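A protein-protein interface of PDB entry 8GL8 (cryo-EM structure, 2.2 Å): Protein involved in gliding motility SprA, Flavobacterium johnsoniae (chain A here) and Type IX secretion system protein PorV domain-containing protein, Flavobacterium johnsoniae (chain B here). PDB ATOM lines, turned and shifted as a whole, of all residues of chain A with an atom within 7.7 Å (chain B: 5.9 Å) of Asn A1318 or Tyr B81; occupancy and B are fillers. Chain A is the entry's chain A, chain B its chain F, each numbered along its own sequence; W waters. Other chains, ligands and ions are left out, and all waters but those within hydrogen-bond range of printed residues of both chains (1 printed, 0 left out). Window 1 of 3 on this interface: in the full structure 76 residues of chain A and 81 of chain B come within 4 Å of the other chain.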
ATOM      1  N   PHE A 199      -6.694 -35.560   6.878  1.00  0.00           N
ATOM      2  CA  PHE A 199      -7.714 -34.516   6.942  1.00  0.00           C
ATOM      3  C   PHE A 199      -8.991 -34.669   6.101  1.00  0.00           C
ATOM      4  O   PHE A 199     -10.055 -34.894   6.684  1.00  0.00           O
ATOM      5  CB  PHE A 199      -6.984 -33.180   6.699  1.00  0.00           C
ATOM      6  CG  PHE A 199      -6.062 -33.171   5.490  1.00  0.00           C
ATOM      7  CD1 PHE A 199      -6.480 -33.536   4.226  1.00  0.00           C
ATOM      8  CD2 PHE A 199      -4.725 -32.844   5.663  1.00  0.00           C
ATOM      9  CE1 PHE A 199      -5.615 -33.542   3.165  1.00  0.00           C
ATOM     10  CE2 PHE A 199      -3.854 -32.851   4.600  1.00  0.00           C
ATOM     11  CZ  PHE A 199      -4.303 -33.207   3.349  1.00  0.00           C
ATOM     12  N   ALA A 950     -21.577 -20.000  23.092  1.00  0.00           N
ATOM     13  CA  ALA A 950     -22.066 -21.286  22.619  1.00  0.00           C
ATOM     14  C   ALA A 950     -22.667 -22.082  23.770  1.00  0.00           C
ATOM     15  O   ALA A 950     -22.182 -22.032  24.903  1.00  0.00           O
ATOM     16  CB  ALA A 950     -20.934 -22.073  21.963  1.00  0.00           C
ATOM     17  N   GLN A 951     -23.740 -22.811  23.473  1.00  0.00           N
ATOM     18  CA  GLN A 951     -24.409 -23.611  24.489  1.00  0.00           C
ATOM     19  C   GLN A 951     -23.477 -24.695  25.013  1.00  0.00           C
ATOM     20  O   GLN A 951     -22.805 -25.384  24.238  1.00  0.00           O
ATOM     21  CB  GLN A 951     -25.679 -24.235  23.914  1.00  0.00           C
ATOM     22  CG  GLN A 951     -26.716 -23.217  23.481  1.00  0.00           C
ATOM     23  CD  GLN A 951     -27.109 -22.281  24.602  1.00  0.00           C
ATOM     24  OE1 GLN A 951     -27.522 -22.719  25.675  1.00  0.00           O
ATOM     25  NE2 GLN A 951     -26.979 -20.982  24.362  1.00  0.00           N
ATOM     26  N   LEU A1314     -21.070 -16.766  12.750  1.00  0.00           N
ATOM     27  CA  LEU A1314     -20.414 -18.057  12.618  1.00  0.00           C
ATOM     28  C   LEU A1314     -21.204 -19.113  13.379  1.00  0.00           C
ATOM     29  O   LEU A1314     -22.157 -18.812  14.098  1.00  0.00           O
ATOM     30  CB  LEU A1314     -18.968 -18.004  13.125  1.00  0.00           C
ATOM     31  CG  LEU A1314     -18.023 -17.033  12.416  1.00  0.00           C
ATOM     32  CD1 LEU A1314     -16.732 -16.877  13.198  1.00  0.00           C
ATOM     33  CD2 LEU A1314     -17.741 -17.494  10.995  1.00  0.00           C
ATOM     34  N   TYR A1315     -20.804 -20.367  13.200  1.00  0.00           N
ATOM     35  CA  TYR A1315     -21.381 -21.491  13.923  1.00  0.00           C
ATOM     36  C   TYR A1315     -20.313 -22.072  14.838  1.00  0.00           C
ATOM     37  O   TYR A1315     -19.308 -22.607  14.360  1.00  0.00           O
ATOM     38  CB  TYR A1315     -21.905 -22.554  12.958  1.00  0.00           C
ATOM     39  CG  TYR A1315     -23.379 -22.434  12.654  1.00  0.00           C
ATOM     40  CD1 TYR A1315     -24.333 -22.756  13.610  1.00  0.00           C
ATOM     41  CD2 TYR A1315     -23.819 -21.995  11.413  1.00  0.00           C
ATOM     42  CE1 TYR A1315     -25.681 -22.646  13.338  1.00  0.00           C
ATOM     43  CE2 TYR A1315     -25.165 -21.881  11.132  1.00  0.00           C
ATOM     44  CZ  TYR A1315     -26.093 -22.208  12.098  1.00  0.00           C
ATOM     45  OH  TYR A1315     -27.436 -22.097  11.823  1.00  0.00           O
ATOM     46  N   ASN A1316     -20.527 -21.963  16.151  1.00  0.00           N
ATOM     47  CA  ASN A1316     -19.551 -22.488  17.100  1.00  0.00           C
ATOM     48  C   ASN A1316     -19.723 -23.991  17.283  1.00  0.00           C
ATOM     49  O   ASN A1316     -18.829 -24.777  16.954  1.00  0.00           O
ATOM     50  CB  ASN A1316     -19.676 -21.760  18.440  1.00  0.00           C
ATOM     51  CG  ASN A1316     -18.361 -21.682  19.182  1.00  0.00           C
ATOM     52  OD1 ASN A1316     -17.545 -22.601  19.119  1.00  0.00           O
ATOM     53  ND2 ASN A1316     -18.147 -20.583  19.892  1.00  0.00           N
ATOM     54  N   ASN A1317     -20.871 -24.406  17.815  1.00  0.00           N
ATOM     55  CA  ASN A1317     -21.276 -25.811  17.788  1.00  0.00           C
ATOM     56  C   ASN A1317     -22.805 -25.821  17.732  1.00  0.00           C
ATOM     57  O   ASN A1317     -23.479 -25.810  18.765  1.00  0.00           O
ATOM     58  CB  ASN A1317     -20.734 -26.585  18.982  1.00  0.00           C
ATOM     59  CG  ASN A1317     -21.040 -25.915  20.306  1.00  0.00           C
ATOM     60  OD1 ASN A1317     -20.347 -24.986  20.719  1.00  0.00           O
ATOM     61  ND2 ASN A1317     -22.084 -26.383  20.981  1.00  0.00           N
ATOM     62  N   ASN A1318     -23.335 -25.844  16.510  1.00  0.00           N
ATOM     63  CA  ASN A1318     -24.770 -25.763  16.247  1.00  0.00           C
ATOM     64  C   ASN A1318     -25.408 -24.524  16.874  1.00  0.00           C
ATOM     65  O   ASN A1318     -26.621 -24.490  17.094  1.00  0.00           O
ATOM     66  CB  ASN A1318     -25.487 -27.033  16.716  1.00  0.00           C
ATOM     67  CG  ASN A1318     -24.614 -28.267  16.595  1.00  0.00           C
ATOM     68  OD1 ASN A1318     -24.197 -28.639  15.499  1.00  0.00           O
ATOM     69  ND2 ASN A1318     -24.320 -28.899  17.724  1.00  0.00           N
ATOM     70  N   THR A1319     -24.606 -23.501  17.162  1.00  0.00           N
ATOM     71  CA  THR A1319     -25.080 -22.257  17.751  1.00  0.00           C
ATOM     72  C   THR A1319     -24.590 -21.092  16.907  1.00  0.00           C
ATOM     73  O   THR A1319     -23.407 -21.032  16.556  1.00  0.00           O
ATOM     74  CB  THR A1319     -24.592 -22.102  19.198  1.00  0.00           C
ATOM     75  OG1 THR A1319     -24.968 -23.253  19.962  1.00  0.00           O
ATOM     76  CG2 THR A1319     -25.193 -20.860  19.838  1.00  0.00           C
ATOM     77  N   VAL A1320     -25.493 -20.171  16.585  1.00  0.00           N
ATOM     78  CA  VAL A1320     -25.132 -18.984  15.817  1.00  0.00           C
ATOM     79  C   VAL A1320     -24.486 -17.975  16.757  1.00  0.00           C
ATOM     80  O   VAL A1320     -25.069 -17.601  17.780  1.00  0.00           O
ATOM     81  CB  VAL A1320     -26.357 -18.381  15.117  1.00  0.00           C
ATOM     82  CG1 VAL A1320     -25.960 -17.137  14.335  1.00  0.00           C
ATOM     83  CG2 VAL A1320     -27.000 -19.406  14.201  1.00  0.00           C
ATOM     84  N   ILE A1321     -23.279 -17.538  16.414  1.00  0.00           N
ATOM     85  CA  ILE A1321     -22.522 -16.577  17.204  1.00  0.00           C
ATOM     86  C   ILE A1321     -22.328 -15.326  16.362  1.00  0.00           C
ATOM     87  O   ILE A1321     -21.765 -15.391  15.260  1.00  0.00           O
ATOM     88  CB  ILE A1321     -21.168 -17.146  17.656  1.00  0.00           C
ATOM     89  CG1 ILE A1321     -21.352 -18.521  18.302  1.00  0.00           C
ATOM     90  CG2 ILE A1321     -20.471 -16.179  18.603  1.00  0.00           C
ATOM     91  CD1 ILE A1321     -21.811 -18.473  19.745  1.00  0.00           C
ATOM     92  N   PRO B  31     -28.036 -27.971  21.421  1.00  0.00           N
ATOM     93  CA  PRO B  31     -28.453 -27.970  20.008  1.00  0.00           C
ATOM     94  C   PRO B  31     -27.959 -29.171  19.213  1.00  0.00           C
ATOM     95  O   PRO B  31     -28.490 -29.422  18.123  1.00  0.00           O
ATOM     96  CB  PRO B  31     -27.856 -26.664  19.468  1.00  0.00           C
ATOM     97  CG  PRO B  31     -26.729 -26.353  20.381  1.00  0.00           C
ATOM     98  CD  PRO B  31     -27.132 -26.852  21.733  1.00  0.00           C
ATOM     99  N   PHE B  32     -26.980 -29.924  19.722  1.00  0.00           N
ATOM    100  CA  PHE B  32     -26.490 -31.100  19.011  1.00  0.00           C
ATOM    101  C   PHE B  32     -27.577 -32.147  18.809  1.00  0.00           C
ATOM    102  O   PHE B  32     -27.430 -33.017  17.946  1.00  0.00           O
ATOM    103  CB  PHE B  32     -25.295 -31.705  19.757  1.00  0.00           C
ATOM    104  CG  PHE B  32     -25.668 -32.765  20.759  1.00  0.00           C
ATOM    105  CD1 PHE B  32     -26.129 -32.416  22.018  1.00  0.00           C
ATOM    106  CD2 PHE B  32     -25.539 -34.110  20.450  1.00  0.00           C
ATOM    107  CE1 PHE B  32     -26.467 -33.385  22.942  1.00  0.00           C
ATOM    108  CE2 PHE B  32     -25.878 -35.083  21.371  1.00  0.00           C
ATOM    109  CZ  PHE B  32     -26.340 -34.720  22.618  1.00  0.00           C
ATOM    110  N   LEU B  33     -28.663 -32.081  19.583  1.00  0.00           N
ATOM    111  CA  LEU B  33     -29.786 -32.989  19.386  1.00  0.00           C
ATOM    112  C   LEU B  33     -30.495 -32.762  18.058  1.00  0.00           C
ATOM    113  O   LEU B  33     -31.220 -33.651  17.601  1.00  0.00           O
ATOM    114  CB  LEU B  33     -30.787 -32.840  20.532  1.00  0.00           C
ATOM    115  CG  LEU B  33     -30.341 -33.347  21.903  1.00  0.00           C
ATOM    116  CD1 LEU B  33     -31.428 -33.115  22.935  1.00  0.00           C
ATOM    117  CD2 LEU B  33     -29.974 -34.813  21.824  1.00  0.00           C
ATOM    118  N   VAL B  35     -28.971 -32.194  15.123  1.00  0.00           N
ATOM    119  CA  VAL B  35     -28.106 -32.551  14.006  1.00  0.00           C
ATOM    120  C   VAL B  35     -28.466 -33.950  13.527  1.00  0.00           C
ATOM    121  O   VAL B  35     -28.625 -34.871  14.337  1.00  0.00           O
ATOM    122  CB  VAL B  35     -26.626 -32.470  14.414  1.00  0.00           C
ATOM    123  CG1 VAL B  35     -25.727 -32.874  13.256  1.00  0.00           C
ATOM    124  CG2 VAL B  35     -26.288 -31.071  14.896  1.00  0.00           C
ATOM    125  N   THR B  79     -20.355 -38.918  11.765  1.00  0.00           N
ATOM    126  CA  THR B  79     -20.443 -37.593  11.152  1.00  0.00           C
ATOM    127  C   THR B  79     -19.238 -36.787  11.608  1.00  0.00           C
ATOM    128  O   THR B  79     -19.230 -36.263  12.736  1.00  0.00           O
ATOM    129  CB  THR B  79     -21.740 -36.887  11.546  1.00  0.00           C
ATOM    130  OG1 THR B  79     -22.862 -37.666  11.118  1.00  0.00           O
ATOM    131  CG2 THR B  79     -21.812 -35.505  10.921  1.00  0.00           C
ATOM    132  N   PRO B  80     -18.191 -36.681  10.797  1.00  0.00           N
ATOM    133  CA  PRO B  80     -17.003 -35.940  11.230  1.00  0.00           C
ATOM    134  C   PRO B  80     -17.229 -34.437  11.208  1.00  0.00           C
ATOM    135  O   PRO B  80     -18.045 -33.913  10.446  1.00  0.00           O
ATOM    136  CB  PRO B  80     -15.936 -36.360  10.216  1.00  0.00           C
ATOM    137  CG  PRO B  80     -16.696 -36.727   8.998  1.00  0.00           C
ATOM    138  CD  PRO B  80     -18.052 -37.217   9.432  1.00  0.00           C
ATOM    139  N   TYR B  81     -16.487 -33.743  12.065  1.00  0.00           N
ATOM    140  CA  TYR B  81     -16.519 -32.292  12.158  1.00  0.00           C
ATOM    141  C   TYR B  81     -15.120 -31.742  11.932  1.00  0.00           C
ATOM    142  O   TYR B  81     -14.148 -32.256  12.495  1.00  0.00           O
ATOM    143  CB  TYR B  81     -17.037 -31.830  13.522  1.00  0.00           C
ATOM    144  CG  TYR B  81     -18.539 -31.781  13.638  1.00  0.00           C
ATOM    145  CD1 TYR B  81     -19.273 -32.934  13.879  1.00  0.00           C
ATOM    146  CD2 TYR B  81     -19.224 -30.582  13.517  1.00  0.00           C
ATOM    147  CE1 TYR B  81     -20.646 -32.894  13.988  1.00  0.00           C
ATOM    148  CE2 TYR B  81     -20.598 -30.532  13.626  1.00  0.00           C
ATOM    149  CZ  TYR B  81     -21.305 -31.691  13.862  1.00  0.00           C
ATOM    150  OH  TYR B  81     -22.673 -31.645  13.971  1.00  0.00           O
ATOM    151  N   LEU B  82     -15.028 -30.696  11.115  1.00  0.00           N
ATOM    152  CA  LEU B  82     -13.765 -30.022  10.815  1.00  0.00           C
ATOM    153  C   LEU B  82     -12.718 -31.021  10.331  1.00  0.00           C
ATOM    154  O   LEU B  82     -11.636 -31.163  10.904  1.00  0.00           O
ATOM    155  CB  LEU B  82     -13.255 -29.250  12.033  1.00  0.00           C
ATOM    156  CG  LEU B  82     -14.227 -28.297  12.722  1.00  0.00           C
ATOM    157  CD1 LEU B  82     -13.826 -28.145  14.173  1.00  0.00           C
ATOM    158  CD2 LEU B  82     -14.250 -26.950  12.023  1.00  0.00           C
ATOM    159  N   THR B  83     -13.067 -31.729   9.255  1.00  0.00           N
ATOM    160  CA  THR B  83     -12.204 -32.796   8.760  1.00  0.00           C
ATOM    161  C   THR B  83     -10.836 -32.261   8.356  1.00  0.00           C
ATOM    162  O   THR B  83      -9.807 -32.873   8.665  1.00  0.00           O
ATOM    163  CB  THR B  83     -12.871 -33.506   7.584  1.00  0.00           C
ATOM    164  OG1 THR B  83     -13.856 -32.645   6.998  1.00  0.00           O
ATOM    165  CG2 THR B  83     -13.538 -34.785   8.050  1.00  0.00           C
ATOM    166  N   ALA B  86      -8.955 -31.041  12.006  1.00  0.00           N
ATOM    167  CA  ALA B  86      -8.542 -32.006  13.013  1.00  0.00           C
ATOM    168  C   ALA B  86      -9.331 -33.296  12.853  1.00  0.00           C
ATOM    169  O   ALA B  86     -10.349 -33.350  12.160  1.00  0.00           O
ATOM    170  CB  ALA B  86      -8.716 -31.445  14.429  1.00  0.00           C
ATOM    171  N   ASN B  87      -8.837 -34.342  13.505  1.00  0.00           N
ATOM    172  CA  ASN B  87      -9.509 -35.628  13.581  1.00  0.00           C
ATOM    173  C   ASN B  87     -10.190 -35.784  14.937  1.00  0.00           C
ATOM    174  O   ASN B  87     -10.018 -34.974  15.849  1.00  0.00           O
ATOM    175  CB  ASN B  87      -8.512 -36.770  13.355  1.00  0.00           C
ATOM    176  CG  ASN B  87      -8.261 -37.045  11.887  1.00  0.00           C
ATOM    177  OD1 ASN B  87      -9.098 -36.751  11.035  1.00  0.00           O
ATOM    178  ND2 ASN B  87      -7.102 -37.617  11.584  1.00  0.00           N
ATOM    179  N   ILE B  89     -12.979 -35.252  16.133  1.00  0.00           N
ATOM    180  CA  ILE B  89     -14.108 -34.395  16.480  1.00  0.00           C
ATOM    181  C   ILE B  89     -15.288 -34.844  15.629  1.00  0.00           C
ATOM    182  O   ILE B  89     -15.338 -34.564  14.429  1.00  0.00           O
ATOM    183  CB  ILE B  89     -13.791 -32.913  16.251  1.00  0.00           C
ATOM    184  CG1 ILE B  89     -12.578 -32.488  17.077  1.00  0.00           C
ATOM    185  CG2 ILE B  89     -14.998 -32.056  16.593  1.00  0.00           C
ATOM    186  CD1 ILE B  89     -11.931 -31.214  16.589  1.00  0.00           C
ATOM    187  N   SER B  90     -16.236 -35.548  16.239  1.00  0.00           N
ATOM    188  CA  SER B  90     -17.284 -36.163  15.440  1.00  0.00           C
ATOM    189  C   SER B  90     -18.521 -36.418  16.285  1.00  0.00           C
ATOM    190  O   SER B  90     -18.472 -36.436  17.520  1.00  0.00           O
ATOM    191  CB  SER B  90     -16.801 -37.473  14.808  1.00  0.00           C
ATOM    192  OG  SER B  90     -16.744 -38.511  15.769  1.00  0.00           O
ATOM    193  N   LEU B  91     -19.634 -36.619  15.584  1.00  0.00           N
ATOM    194  CA  LEU B  91     -20.890 -37.076  16.164  1.00  0.00           C
ATOM    195  C   LEU B  91     -21.116 -38.511  15.704  1.00  0.00           C
ATOM    196  O   LEU B  91     -21.283 -38.768  14.508  1.00  0.00           O
ATOM    197  CB  LEU B  91     -22.045 -36.169  15.748  1.00  0.00           C
ATOM    198  CG  LEU B  91     -23.461 -36.690  15.999  1.00  0.00           C
ATOM    199  CD1 LEU B  91     -23.813 -36.616  17.476  1.00  0.00           C
ATOM    200  CD2 LEU B  91     -24.468 -35.915  15.165  1.00  0.00           C
ATOM    201  N   PHE B 113     -21.451 -36.790  20.764  1.00  0.00           N
ATOM    202  CA  PHE B 113     -20.604 -35.796  20.123  1.00  0.00           C
ATOM    203  C   PHE B 113     -19.362 -35.598  20.974  1.00  0.00           C
ATOM    204  O   PHE B 113     -19.467 -35.371  22.183  1.00  0.00           O
ATOM    205  CB  PHE B 113     -21.345 -34.471  19.946  1.00  0.00           C
ATOM    206  CG  PHE B 113     -20.498 -33.383  19.361  1.00  0.00           C
ATOM    207  CD1 PHE B 113     -20.082 -33.445  18.043  1.00  0.00           C
ATOM    208  CD2 PHE B 113     -20.107 -32.304  20.132  1.00  0.00           C
ATOM    209  CE1 PHE B 113     -19.297 -32.447  17.504  1.00  0.00           C
ATOM    210  CE2 PHE B 113     -19.323 -31.304  19.599  1.00  0.00           C
ATOM    211  CZ  PHE B 113     -18.918 -31.374  18.282  1.00  0.00           C
ATOM    212  N   GLU B 137     -20.838 -34.778  24.683  1.00  0.00           N
ATOM    213  CA  GLU B 137     -22.263 -34.492  24.817  1.00  0.00           C
ATOM    214  C   GLU B 137     -23.014 -35.692  24.272  1.00  0.00           C
ATOM    215  O   GLU B 137     -22.914 -35.983  23.079  1.00  0.00           O
ATOM    216  CB  GLU B 137     -22.635 -33.225  24.047  1.00  0.00           C
ATOM    217  CG  GLU B 137     -23.566 -32.287  24.778  1.00  0.00           C
ATOM    218  CD  GLU B 137     -23.643 -30.923  24.119  1.00  0.00           C
ATOM    219  OE1 GLU B 137     -23.184 -30.795  22.965  1.00  0.00           O
ATOM    220  OE2 GLU B 137     -24.161 -29.979  24.754  1.00  0.00           O
ATOM    221  N   PRO B 382     -20.957 -26.050   9.205  1.00  0.00           N
ATOM    222  CA  PRO B 382     -19.882 -26.853   9.813  1.00  0.00           C
ATOM    223  C   PRO B 382     -19.728 -28.235   9.202  1.00  0.00           C
ATOM    224  O   PRO B 382     -18.683 -28.866   9.397  1.00  0.00           O
ATOM    225  CB  PRO B 382     -20.296 -26.936  11.289  1.00  0.00           C
ATOM    226  CG  PRO B 382     -21.765 -26.680  11.290  1.00  0.00           C
ATOM    227  CD  PRO B 382     -22.019 -25.721  10.169  1.00  0.00           C
ATOM    228  N   LEU B 383     -20.728 -28.725   8.472  1.00  0.00           N
ATOM    229  CA  LEU B 383     -20.678 -30.041   7.853  1.00  0.00           C
ATOM    230  C   LEU B 383     -20.371 -29.975   6.360  1.00  0.00           C
ATOM    231  O   LEU B 383     -20.630 -30.941   5.637  1.00  0.00           O
ATOM    232  CB  LEU B 383     -21.991 -30.784   8.096  1.00  0.00           C
ATOM    233  CG  LEU B 383     -22.317 -31.022   9.572  1.00  0.00           C
ATOM    234  CD1 LEU B 383     -23.679 -31.666   9.733  1.00  0.00           C
ATOM    235  CD2 LEU B 383     -21.238 -31.869  10.225  1.00  0.00           C
ATOM    236  N   THR B 386     -17.805 -32.648   3.933  1.00  0.00           N
ATOM    237  CA  THR B 386     -17.793 -33.737   4.899  1.00  0.00           C
ATOM    238  C   THR B 386     -18.591 -34.906   4.347  1.00  0.00           C
ATOM    239  O   THR B 386     -19.709 -34.723   3.856  1.00  0.00           O
ATOM    240  CB  THR B 386     -18.371 -33.280   6.247  1.00  0.00           C
ATOM    241  OG1 THR B 386     -17.374 -32.552   6.975  1.00  0.00           O
ATOM    242  CG2 THR B 386     -18.833 -34.467   7.078  1.00  0.00           C
ATOM    243  N   ARG B 388     -20.476 -38.125   5.421  1.00  0.00           N
ATOM    244  CA  ARG B 388     -21.068 -38.885   6.512  1.00  0.00           C
ATOM    245  C   ARG B 388     -21.151 -40.356   6.140  1.00  0.00           C
ATOM    246  O   ARG B 388     -21.498 -40.700   5.005  1.00  0.00           O
ATOM    247  CB  ARG B 388     -22.466 -38.369   6.837  1.00  0.00           C
ATOM    248  CG  ARG B 388     -22.514 -37.195   7.781  1.00  0.00           C
ATOM    249  CD  ARG B 388     -23.728 -36.345   7.477  1.00  0.00           C
ATOM    250  NE  ARG B 388     -24.412 -35.886   8.678  1.00  0.00           N
ATOM    251  CZ  ARG B 388     -25.075 -34.742   8.764  1.00  0.00           C
ATOM    252  NH1 ARG B 388     -25.170 -33.921   7.732  1.00  0.00           N
ATOM    253  NH2 ARG B 388     -25.658 -34.415   9.913  1.00  0.00           N
HETATM  254  O   HOH W   1     -24.410 -28.618  21.360  1.00  0.00           O
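The side-chain amide nitrogen (ND2) of Asn A1318 sits close to the backbone NH (N) of Phe B32 (3.5 Å).
The backbone carbonyl oxygen (O) of Phe A199 sits close to the backbone carbonyl oxygen (O) of Thr B83 (2.8 Å).
O of Gln A951 lies within hydrogen-bond range of ND2 of Asn A1317 (3.5 Å).
O of Asn A1317 sits at hydrogen-bond distance from OG1 of Thr A1319.
The backbone NH of Tyr B81 lies within hydrogen-bond range of the backbone carbonyl oxygen of Ile B89 (2.8 Å).
Of the printed residues of chain B, Asn A1318 touches Pro B31, Phe B32, Val B35 and Tyr B81.
Tyr B81 touches just one residue of chain A: Asn A1318.
Printed residues of chain A within 4 Å of Val B35: Asn A1318 (3.3 Å).
Printed residues of chain B within 4 Å of Thr A1319: Pro B31.
The nearest residue of chain B that does not touch Asn A1318 is Pro B382 (5.2 Å).
Of the 11 printed residues of chain A, 5 touch a printed residue of chain B.
Printed residues of chain A that touch a printed residue of chain B: Phe A199, Gln A951, Asn A1317, Asn A1318 and Thr A1319.
Hydrophobic or aromatic side chains of chain A that line the printed part of chain B: Phe A199.
Of the 20 printed residues of chain B, 5 touch a printed residue of chain A.
Among the printed residues, 8 pairs touch across the chains.
Among the printed residues, no Asp or Glu carboxylate lies within 4 Å of a Lys or Arg side-chain nitrogen of the other chain.
Among the printed residues, merely in contact across the chains: Gln A951 with Pro B31, Asn A1317 with Pro B31, Asn A1318 with Pro B31, Asn A1318 with Val B35, Asn A1318 with Tyr B81 and Thr A1319 with Pro B31.
Water W1 lies within hydrogen-bond range of OE1 of Glu B137 (3.0 Å), ND2 of Asn A1317 (3.2 Å) and N of Phe B32 (3.3 Å).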
